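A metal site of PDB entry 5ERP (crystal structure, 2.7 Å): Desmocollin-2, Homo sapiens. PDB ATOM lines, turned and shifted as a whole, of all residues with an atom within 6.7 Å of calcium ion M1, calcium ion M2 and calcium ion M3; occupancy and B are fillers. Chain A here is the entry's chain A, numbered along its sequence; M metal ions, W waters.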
ATOM      1  N   GLU A 247     -38.852 -23.673 -27.063  1.00  0.00           N
ATOM      2  CA  GLU A 247     -38.205 -23.185 -28.274  1.00  0.00           C
ATOM      3  C   GLU A 247     -38.831 -23.760 -29.541  1.00  0.00           C
ATOM      4  O   GLU A 247     -38.857 -23.110 -30.579  1.00  0.00           O
ATOM      5  CB  GLU A 247     -36.714 -23.549 -28.223  1.00  0.00           C
ATOM      6  CG  GLU A 247     -35.965 -23.432 -29.538  1.00  0.00           C
ATOM      7  CD  GLU A 247     -34.595 -24.079 -29.486  1.00  0.00           C
ATOM      8  OE1 GLU A 247     -34.147 -24.439 -28.371  1.00  0.00           O
ATOM      9  OE2 GLU A 247     -33.977 -24.237 -30.554  1.00  0.00           O
ATOM     10  N   LEU A 298     -39.799 -20.143 -33.132  1.00  0.00           N
ATOM     11  CA  LEU A 298     -38.758 -19.563 -32.297  1.00  0.00           C
ATOM     12  C   LEU A 298     -37.453 -20.332 -32.487  1.00  0.00           C
ATOM     13  O   LEU A 298     -37.445 -21.460 -32.980  1.00  0.00           O
ATOM     14  CB  LEU A 298     -39.181 -19.579 -30.824  1.00  0.00           C
ATOM     15  CG  LEU A 298     -40.616 -19.113 -30.544  1.00  0.00           C
ATOM     16  CD1 LEU A 298     -40.936 -19.185 -29.056  1.00  0.00           C
ATOM     17  CD2 LEU A 298     -40.859 -17.712 -31.083  1.00  0.00           C
ATOM     18  N   ASP A 299     -36.348 -19.710 -32.079  1.00  0.00           N
ATOM     19  CA  ASP A 299     -35.031 -20.324 -32.148  1.00  0.00           C
ATOM     20  C   ASP A 299     -34.157 -19.770 -31.039  1.00  0.00           C
ATOM     21  O   ASP A 299     -33.738 -18.617 -31.083  1.00  0.00           O
ATOM     22  CB  ASP A 299     -34.383 -20.074 -33.513  1.00  0.00           C
ATOM     23  CG  ASP A 299     -33.005 -20.698 -33.633  1.00  0.00           C
ATOM     24  OD1 ASP A 299     -32.724 -21.680 -32.910  1.00  0.00           O
ATOM     25  OD2 ASP A 299     -32.198 -20.191 -34.431  1.00  0.00           O
ATOM     26  N   ARG A 300     -33.880 -20.593 -30.027  1.00  0.00           N
ATOM     27  CA  ARG A 300     -33.058 -20.165 -28.903  1.00  0.00           C
ATOM     28  C   ARG A 300     -31.653 -19.813 -29.357  1.00  0.00           C
ATOM     29  O   ARG A 300     -30.999 -18.954 -28.770  1.00  0.00           O
ATOM     30  CB  ARG A 300     -33.017 -21.252 -27.822  1.00  0.00           C
ATOM     31  CG  ARG A 300     -32.113 -20.933 -26.641  1.00  0.00           C
ATOM     32  CD  ARG A 300     -32.030 -22.082 -25.670  1.00  0.00           C
ATOM     33  NE  ARG A 300     -30.889 -21.960 -24.761  1.00  0.00           N
ATOM     34  CZ  ARG A 300     -29.632 -22.233 -25.088  1.00  0.00           C
ATOM     35  NH1 ARG A 300     -29.331 -22.652 -26.312  1.00  0.00           N
ATOM     36  NH2 ARG A 300     -28.670 -22.085 -24.184  1.00  0.00           N
ATOM     37  N   GLU A 301     -31.200 -20.461 -30.424  1.00  0.00           N
ATOM     38  CA  GLU A 301     -29.815 -20.331 -30.866  1.00  0.00           C
ATOM     39  C   GLU A 301     -29.623 -19.279 -31.959  1.00  0.00           C
ATOM     40  O   GLU A 301     -28.539 -19.161 -32.520  1.00  0.00           O
ATOM     41  CB  GLU A 301     -29.311 -21.689 -31.370  1.00  0.00           C
ATOM     42  CG  GLU A 301     -29.317 -22.762 -30.295  1.00  0.00           C
ATOM     43  CD  GLU A 301     -30.691 -23.361 -30.075  1.00  0.00           C
ATOM     44  OE1 GLU A 301     -31.484 -23.414 -31.044  1.00  0.00           O
ATOM     45  OE2 GLU A 301     -30.978 -23.772 -28.939  1.00  0.00           O
ATOM     46  N   ALA A 302     -30.682 -18.528 -32.265  1.00  0.00           N
ATOM     47  CA  ALA A 302     -30.594 -17.454 -33.246  1.00  0.00           C
ATOM     48  C   ALA A 302     -29.616 -16.384 -32.770  1.00  0.00           C
ATOM     49  O   ALA A 302     -29.376 -16.257 -31.560  1.00  0.00           O
ATOM     50  CB  ALA A 302     -31.961 -16.851 -33.508  1.00  0.00           C
ATOM     51  N   GLN A 333     -37.031 -22.049 -23.577  1.00  0.00           N
ATOM     52  CA  GLN A 333     -36.525 -23.259 -22.948  1.00  0.00           C
ATOM     53  C   GLN A 333     -35.922 -24.112 -24.049  1.00  0.00           C
ATOM     54  O   GLN A 333     -36.583 -24.413 -25.047  1.00  0.00           O
ATOM     55  CB  GLN A 333     -37.631 -23.998 -22.191  1.00  0.00           C
ATOM     56  CG  GLN A 333     -37.139 -25.188 -21.389  1.00  0.00           C
ATOM     57  CD  GLN A 333     -38.255 -25.913 -20.671  1.00  0.00           C
ATOM     58  OE1 GLN A 333     -39.379 -25.417 -20.586  1.00  0.00           O
ATOM     59  NE2 GLN A 333     -37.938 -27.071 -20.104  1.00  0.00           N
ATOM     60  N   ASP A 334     -34.666 -24.501 -23.876  1.00  0.00           N
ATOM     61  CA  ASP A 334     -33.934 -25.180 -24.926  1.00  0.00           C
ATOM     62  C   ASP A 334     -34.456 -26.579 -25.236  1.00  0.00           C
ATOM     63  O   ASP A 334     -34.932 -27.286 -24.356  1.00  0.00           O
ATOM     64  CB  ASP A 334     -32.450 -25.288 -24.582  1.00  0.00           C
ATOM     65  CG  ASP A 334     -31.631 -25.884 -25.703  1.00  0.00           C
ATOM     66  OD1 ASP A 334     -31.727 -25.389 -26.840  1.00  0.00           O
ATOM     67  OD2 ASP A 334     -30.915 -26.875 -25.454  1.00  0.00           O
ATOM     68  N   VAL A 335     -34.358 -26.934 -26.515  1.00  0.00           N
ATOM     69  CA  VAL A 335     -34.674 -28.269 -26.981  1.00  0.00           C
ATOM     70  C   VAL A 335     -33.462 -28.730 -27.795  1.00  0.00           C
ATOM     71  O   VAL A 335     -32.991 -28.001 -28.666  1.00  0.00           O
ATOM     72  CB  VAL A 335     -35.946 -28.278 -27.862  1.00  0.00           C
ATOM     73  CG1 VAL A 335     -36.215 -29.653 -28.439  1.00  0.00           C
ATOM     74  CG2 VAL A 335     -37.150 -27.786 -27.054  1.00  0.00           C
ATOM     75  N   ASN A 336     -32.947 -29.927 -27.503  1.00  0.00           N
ATOM     76  CA  ASN A 336     -31.765 -30.403 -28.198  1.00  0.00           C
ATOM     77  C   ASN A 336     -32.081 -30.650 -29.671  1.00  0.00           C
ATOM     78  O   ASN A 336     -32.453 -31.755 -30.071  1.00  0.00           O
ATOM     79  CB  ASN A 336     -31.208 -31.678 -27.559  1.00  0.00           C
ATOM     80  CG  ASN A 336     -29.787 -31.978 -28.008  1.00  0.00           C
ATOM     81  OD1 ASN A 336     -29.377 -31.614 -29.108  1.00  0.00           O
ATOM     82  ND2 ASN A 336     -29.026 -32.653 -27.156  1.00  0.00           N
ATOM     83  N   ASP A 337     -31.914 -29.601 -30.472  1.00  0.00           N
ATOM     84  CA  ASP A 337     -32.213 -29.651 -31.902  1.00  0.00           C
ATOM     85  C   ASP A 337     -31.016 -29.176 -32.714  1.00  0.00           C
ATOM     86  O   ASP A 337     -31.167 -28.799 -33.878  1.00  0.00           O
ATOM     87  CB  ASP A 337     -33.443 -28.812 -32.217  1.00  0.00           C
ATOM     88  CG  ASP A 337     -33.277 -27.341 -31.842  1.00  0.00           C
ATOM     89  OD1 ASP A 337     -32.225 -26.988 -31.260  1.00  0.00           O
ATOM     90  OD2 ASP A 337     -34.195 -26.546 -32.139  1.00  0.00           O
ATOM     91  N   ASN A 338     -29.840 -29.175 -32.096  1.00  0.00           N
ATOM     92  CA  ASN A 338     -28.626 -28.750 -32.776  1.00  0.00           C
ATOM     93  C   ASN A 338     -27.457 -29.703 -32.555  1.00  0.00           C
ATOM     94  O   ASN A 338     -27.191 -30.149 -31.438  1.00  0.00           O
ATOM     95  CB  ASN A 338     -28.226 -27.344 -32.315  1.00  0.00           C
ATOM     96  CG  ASN A 338     -29.153 -26.273 -32.860  1.00  0.00           C
ATOM     97  OD1 ASN A 338     -29.653 -25.432 -32.115  1.00  0.00           O
ATOM     98  ND2 ASN A 338     -29.405 -26.305 -34.157  1.00  0.00           N
ATOM     99  N   SER A 339     -26.763 -30.011 -33.642  1.00  0.00           N
ATOM    100  CA  SER A 339     -25.562 -30.836 -33.631  1.00  0.00           C
ATOM    101  C   SER A 339     -24.328 -29.976 -33.398  1.00  0.00           C
ATOM    102  O   SER A 339     -24.396 -28.751 -33.511  1.00  0.00           O
ATOM    103  CB  SER A 339     -25.431 -31.604 -34.949  1.00  0.00           C
ATOM    104  OG  SER A 339     -25.672 -30.745 -36.050  1.00  0.00           O
ATOM    105  N   PRO A 340     -23.193 -30.609 -33.054  1.00  0.00           N
ATOM    106  CA  PRO A 340     -21.946 -29.849 -32.875  1.00  0.00           C
ATOM    107  C   PRO A 340     -21.521 -29.125 -34.153  1.00  0.00           C
ATOM    108  O   PRO A 340     -22.095 -29.363 -35.214  1.00  0.00           O
ATOM    109  CB  PRO A 340     -20.921 -30.938 -32.510  1.00  0.00           C
ATOM    110  CG  PRO A 340     -21.741 -32.060 -31.963  1.00  0.00           C
ATOM    111  CD  PRO A 340     -23.036 -32.034 -32.710  1.00  0.00           C
ATOM    112  N   ASP A 363     -21.434 -26.676 -29.325  1.00  0.00           N
ATOM    113  CA  ASP A 363     -22.845 -27.013 -29.435  1.00  0.00           C
ATOM    114  C   ASP A 363     -23.691 -25.815 -29.006  1.00  0.00           C
ATOM    115  O   ASP A 363     -23.647 -25.412 -27.848  1.00  0.00           O
ATOM    116  CB  ASP A 363     -23.179 -28.241 -28.591  1.00  0.00           C
ATOM    117  CG  ASP A 363     -24.435 -28.949 -29.067  1.00  0.00           C
ATOM    118  OD1 ASP A 363     -25.426 -28.255 -29.395  1.00  0.00           O
ATOM    119  OD2 ASP A 363     -24.426 -30.194 -29.130  1.00  0.00           O
ATOM    120  N   PRO A 364     -24.466 -25.232 -29.948  1.00  0.00           N
ATOM    121  CA  PRO A 364     -25.303 -24.057 -29.646  1.00  0.00           C
ATOM    122  C   PRO A 364     -26.280 -24.274 -28.491  1.00  0.00           C
ATOM    123  O   PRO A 364     -26.638 -23.323 -27.806  1.00  0.00           O
ATOM    124  CB  PRO A 364     -26.053 -23.832 -30.952  1.00  0.00           C
ATOM    125  CG  PRO A 364     -25.176 -24.376 -31.994  1.00  0.00           C
ATOM    126  CD  PRO A 364     -24.533 -25.584 -31.376  1.00  0.00           C
ATOM    127  N   ASP A 365     -26.706 -25.525 -28.288  1.00  0.00           N
ATOM    128  CA  ASP A 365     -27.670 -25.828 -27.237  1.00  0.00           C
ATOM    129  C   ASP A 365     -27.055 -25.636 -25.855  1.00  0.00           C
ATOM    130  O   ASP A 365     -25.868 -25.358 -25.730  1.00  0.00           O
ATOM    131  CB  ASP A 365     -28.179 -27.267 -27.387  1.00  0.00           C
ATOM    132  CG  ASP A 365     -28.875 -27.507 -28.717  1.00  0.00           C
ATOM    133  OD1 ASP A 365     -29.557 -26.584 -29.209  1.00  0.00           O
ATOM    134  OD2 ASP A 365     -28.739 -28.618 -29.261  1.00  0.00           O
ATOM    135  N   GLU A 366     -27.884 -25.789 -24.833  1.00  0.00           N
ATOM    136  CA  GLU A 366     -27.434 -25.640 -23.454  1.00  0.00           C
ATOM    137  C   GLU A 366     -26.502 -26.800 -23.074  1.00  0.00           C
ATOM    138  O   GLU A 366     -26.516 -27.840 -23.739  1.00  0.00           O
ATOM    139  CB  GLU A 366     -28.649 -25.552 -22.524  1.00  0.00           C
ATOM    140  CG  GLU A 366     -29.514 -26.803 -22.475  1.00  0.00           C
ATOM    141  CD  GLU A 366     -30.798 -26.587 -21.705  1.00  0.00           C
ATOM    142  OE1 GLU A 366     -30.858 -25.631 -20.896  1.00  0.00           O
ATOM    143  OE2 GLU A 366     -31.760 -27.359 -21.910  1.00  0.00           O
ATOM    144  N   HIS A 369     -27.339 -30.366 -23.193  1.00  0.00           N
ATOM    145  CA  HIS A 369     -27.595 -30.862 -24.545  1.00  0.00           C
ATOM    146  C   HIS A 369     -26.402 -30.627 -25.463  1.00  0.00           C
ATOM    147  O   HIS A 369     -26.562 -30.316 -26.648  1.00  0.00           O
ATOM    148  CB  HIS A 369     -28.838 -30.191 -25.116  1.00  0.00           C
ATOM    149  CG  HIS A 369     -30.105 -30.570 -24.422  1.00  0.00           C
ATOM    150  ND1 HIS A 369     -31.249 -29.810 -24.486  1.00  0.00           N
ATOM    151  CD2 HIS A 369     -30.404 -31.641 -23.647  1.00  0.00           C
ATOM    152  CE1 HIS A 369     -32.207 -30.391 -23.774  1.00  0.00           C
ATOM    153  NE2 HIS A 369     -31.728 -31.506 -23.259  1.00  0.00           N
ATOM    154  N   GLY A 370     -25.189 -30.774 -24.915  1.00  0.00           N
ATOM    155  CA  GLY A 370     -23.971 -30.561 -25.678  1.00  0.00           C
ATOM    156  C   GLY A 370     -22.896 -31.587 -25.342  1.00  0.00           C
ATOM    157  O   GLY A 370     -23.052 -32.762 -25.654  1.00  0.00           O
ATOM    158  N   PHE A 373     -18.291 -34.334 -26.350  1.00  0.00           N
ATOM    159  CA  PHE A 373     -18.383 -34.655 -27.768  1.00  0.00           C
ATOM    160  C   PHE A 373     -17.559 -35.878 -28.123  1.00  0.00           C
ATOM    161  O   PHE A 373     -16.499 -36.112 -27.542  1.00  0.00           O
ATOM    162  CB  PHE A 373     -17.923 -33.462 -28.611  1.00  0.00           C
ATOM    163  CG  PHE A 373     -18.681 -32.201 -28.345  1.00  0.00           C
ATOM    164  CD1 PHE A 373     -20.033 -32.226 -28.076  1.00  0.00           C
ATOM    165  CD2 PHE A 373     -18.022 -30.979 -28.366  1.00  0.00           C
ATOM    166  CE1 PHE A 373     -20.731 -31.054 -27.825  1.00  0.00           C
ATOM    167  CE2 PHE A 373     -18.707 -29.809 -28.112  1.00  0.00           C
ATOM    168  CZ  PHE A 373     -20.062 -29.851 -27.848  1.00  0.00           C
ATOM    169  N   ASP A 419     -22.726 -35.226 -30.326  1.00  0.00           N
ATOM    170  CA  ASP A 419     -22.871 -34.726 -28.968  1.00  0.00           C
ATOM    171  C   ASP A 419     -23.136 -35.861 -27.985  1.00  0.00           C
ATOM    172  O   ASP A 419     -23.044 -37.033 -28.338  1.00  0.00           O
ATOM    173  CB  ASP A 419     -23.993 -33.687 -28.901  1.00  0.00           C
ATOM    174  CG  ASP A 419     -25.345 -34.262 -29.288  1.00  0.00           C
ATOM    175  OD1 ASP A 419     -25.396 -35.402 -29.793  1.00  0.00           O
ATOM    176  OD2 ASP A 419     -26.365 -33.568 -29.084  1.00  0.00           O
ATOM    177  N   ARG A 420     -23.458 -35.492 -26.750  1.00  0.00           N
ATOM    178  CA  ARG A 420     -23.728 -36.461 -25.693  1.00  0.00           C
ATOM    179  C   ARG A 420     -24.863 -37.422 -26.057  1.00  0.00           C
ATOM    180  O   ARG A 420     -24.862 -38.568 -25.620  1.00  0.00           O
ATOM    181  CB  ARG A 420     -24.069 -35.731 -24.394  1.00  0.00           C
ATOM    182  CG  ARG A 420     -23.967 -36.597 -23.151  1.00  0.00           C
ATOM    183  CD  ARG A 420     -24.325 -35.797 -21.909  1.00  0.00           C
ATOM    184  NE  ARG A 420     -25.719 -35.379 -21.943  1.00  0.00           N
ATOM    185  CZ  ARG A 420     -26.739 -36.135 -21.539  1.00  0.00           C
ATOM    186  NH1 ARG A 420     -26.530 -37.355 -21.075  1.00  0.00           N
ATOM    187  NH2 ARG A 420     -27.982 -35.667 -21.603  1.00  0.00           N
ATOM    188  N   MET A 423     -26.646 -36.338 -31.672  1.00  0.00           N
ATOM    189  CA  MET A 423     -26.863 -35.423 -32.791  1.00  0.00           C
ATOM    190  C   MET A 423     -25.530 -35.242 -33.503  1.00  0.00           C
ATOM    191  O   MET A 423     -24.592 -34.672 -32.938  1.00  0.00           O
ATOM    192  CB  MET A 423     -27.419 -34.079 -32.333  1.00  0.00           C
ATOM    193  CG  MET A 423     -28.899 -34.095 -31.979  1.00  0.00           C
ATOM    194  SD  MET A 423     -29.957 -34.292 -33.439  1.00  0.00           S
ATOM    195  CE  MET A 423     -29.637 -32.761 -34.327  1.00  0.00           C
HETATM  196 CA    CA M   1     -31.929 -25.868 -29.135  1.00  0.00          CA
HETATM  197 CA    CA M   2     -33.348 -24.035 -32.897  1.00  0.00          CA
HETATM  198 CA    CA M   3     -27.038 -30.560 -28.950  1.00  0.00          CA
HETATM  199  O   HOH W   1     -35.446 -23.305 -34.359  1.00  0.00           O
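OD1 of Asn 338 sits close to OE1 of Glu 301 (2.9 Å). OE2 of Glu 301 lies close to NH1 of Arg 300 (3.3 Å). OD2 of Asp 334 is in hydrogen-bond range of ND1 of His 369 (3.1 Å). The side-chain carboxylate of Asp 334 sits close to the guanidinium group of Arg 300. The side-chain carboxylate (OD2) of Asp 334 lies within hydrogen-bond range of the backbone NH (N) of Glu 366 (3.3 Å). O of Gln 333 is in hydrogen-bond range of N of Glu 247 (3.1 Å). The side-chain carboxylate of Asp 419 is in hydrogen-bond range of the side-chain amide nitrogen of Asn 336 (3.4 Å). The side-chain carboxylate of Asp 419 sits at hydrogen-bond distance from the backbone NH of Met 423 (2.4 Å).
The nearest printed residue that does not touch calcium ion M1 is Asn 336 (4.5 Å).
Within 4 Å of calcium ion M2: Glu 247, Asp 299, Glu 301 and Asp 337. The nearest printed residue that does not touch calcium ion M2 is Asn 338 (4.03 Å).
Along chain A the residues within 4 Å of calcium ion M3 span positions 336 to 419. The nearest printed residue that does not touch calcium ion M3 is Gly 370 (4.4 Å).
Calcium ion M1 is bound by the side-chain carboxylate (OE2) of Glu 301, the side-chain carboxylate (OD1) of Asp 334, the side-chain carboxylate (OD1) of Asp 337, the backbone carbonyl oxygen (O) of Val 335, the side-chain carboxylate (OD1) of Asp 365 and the side-chain carboxylate (OE1) of Glu 247. Slightly farther from calcium ion M1 lies OE2 of Glu 247 (3.0 Å). Slightly farther from calcium ion M1 lies OE1 of Glu 301 (3.1 Å).
Calcium ion M2 is bound by the side-chain carboxylate of Glu 247 (2.4 Å), the side-chain carboxylate of Asp 299 (2.4 Å), water W1 (2.7 Å), the side-chain carboxylate of Glu 301 (2.7 Å) and the side-chain carboxylate of Asp 337 (2.8 Å).
Calcium ion M3 is bound by the backbone carbonyl oxygen (O) of His 369, the backbone carbonyl oxygen (O) of Asn 338, the side-chain amide oxygen (OD1) of Asn 336, the side-chain carboxylate (OD2) of Asp 365, the side-chain carboxylate (OD2) of Asp 363 and the side-chain carboxylate (OD1) of Asp 363. Slightly farther from calcium ion M3 lies OD2 of Asp 419 (3.1 Å).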
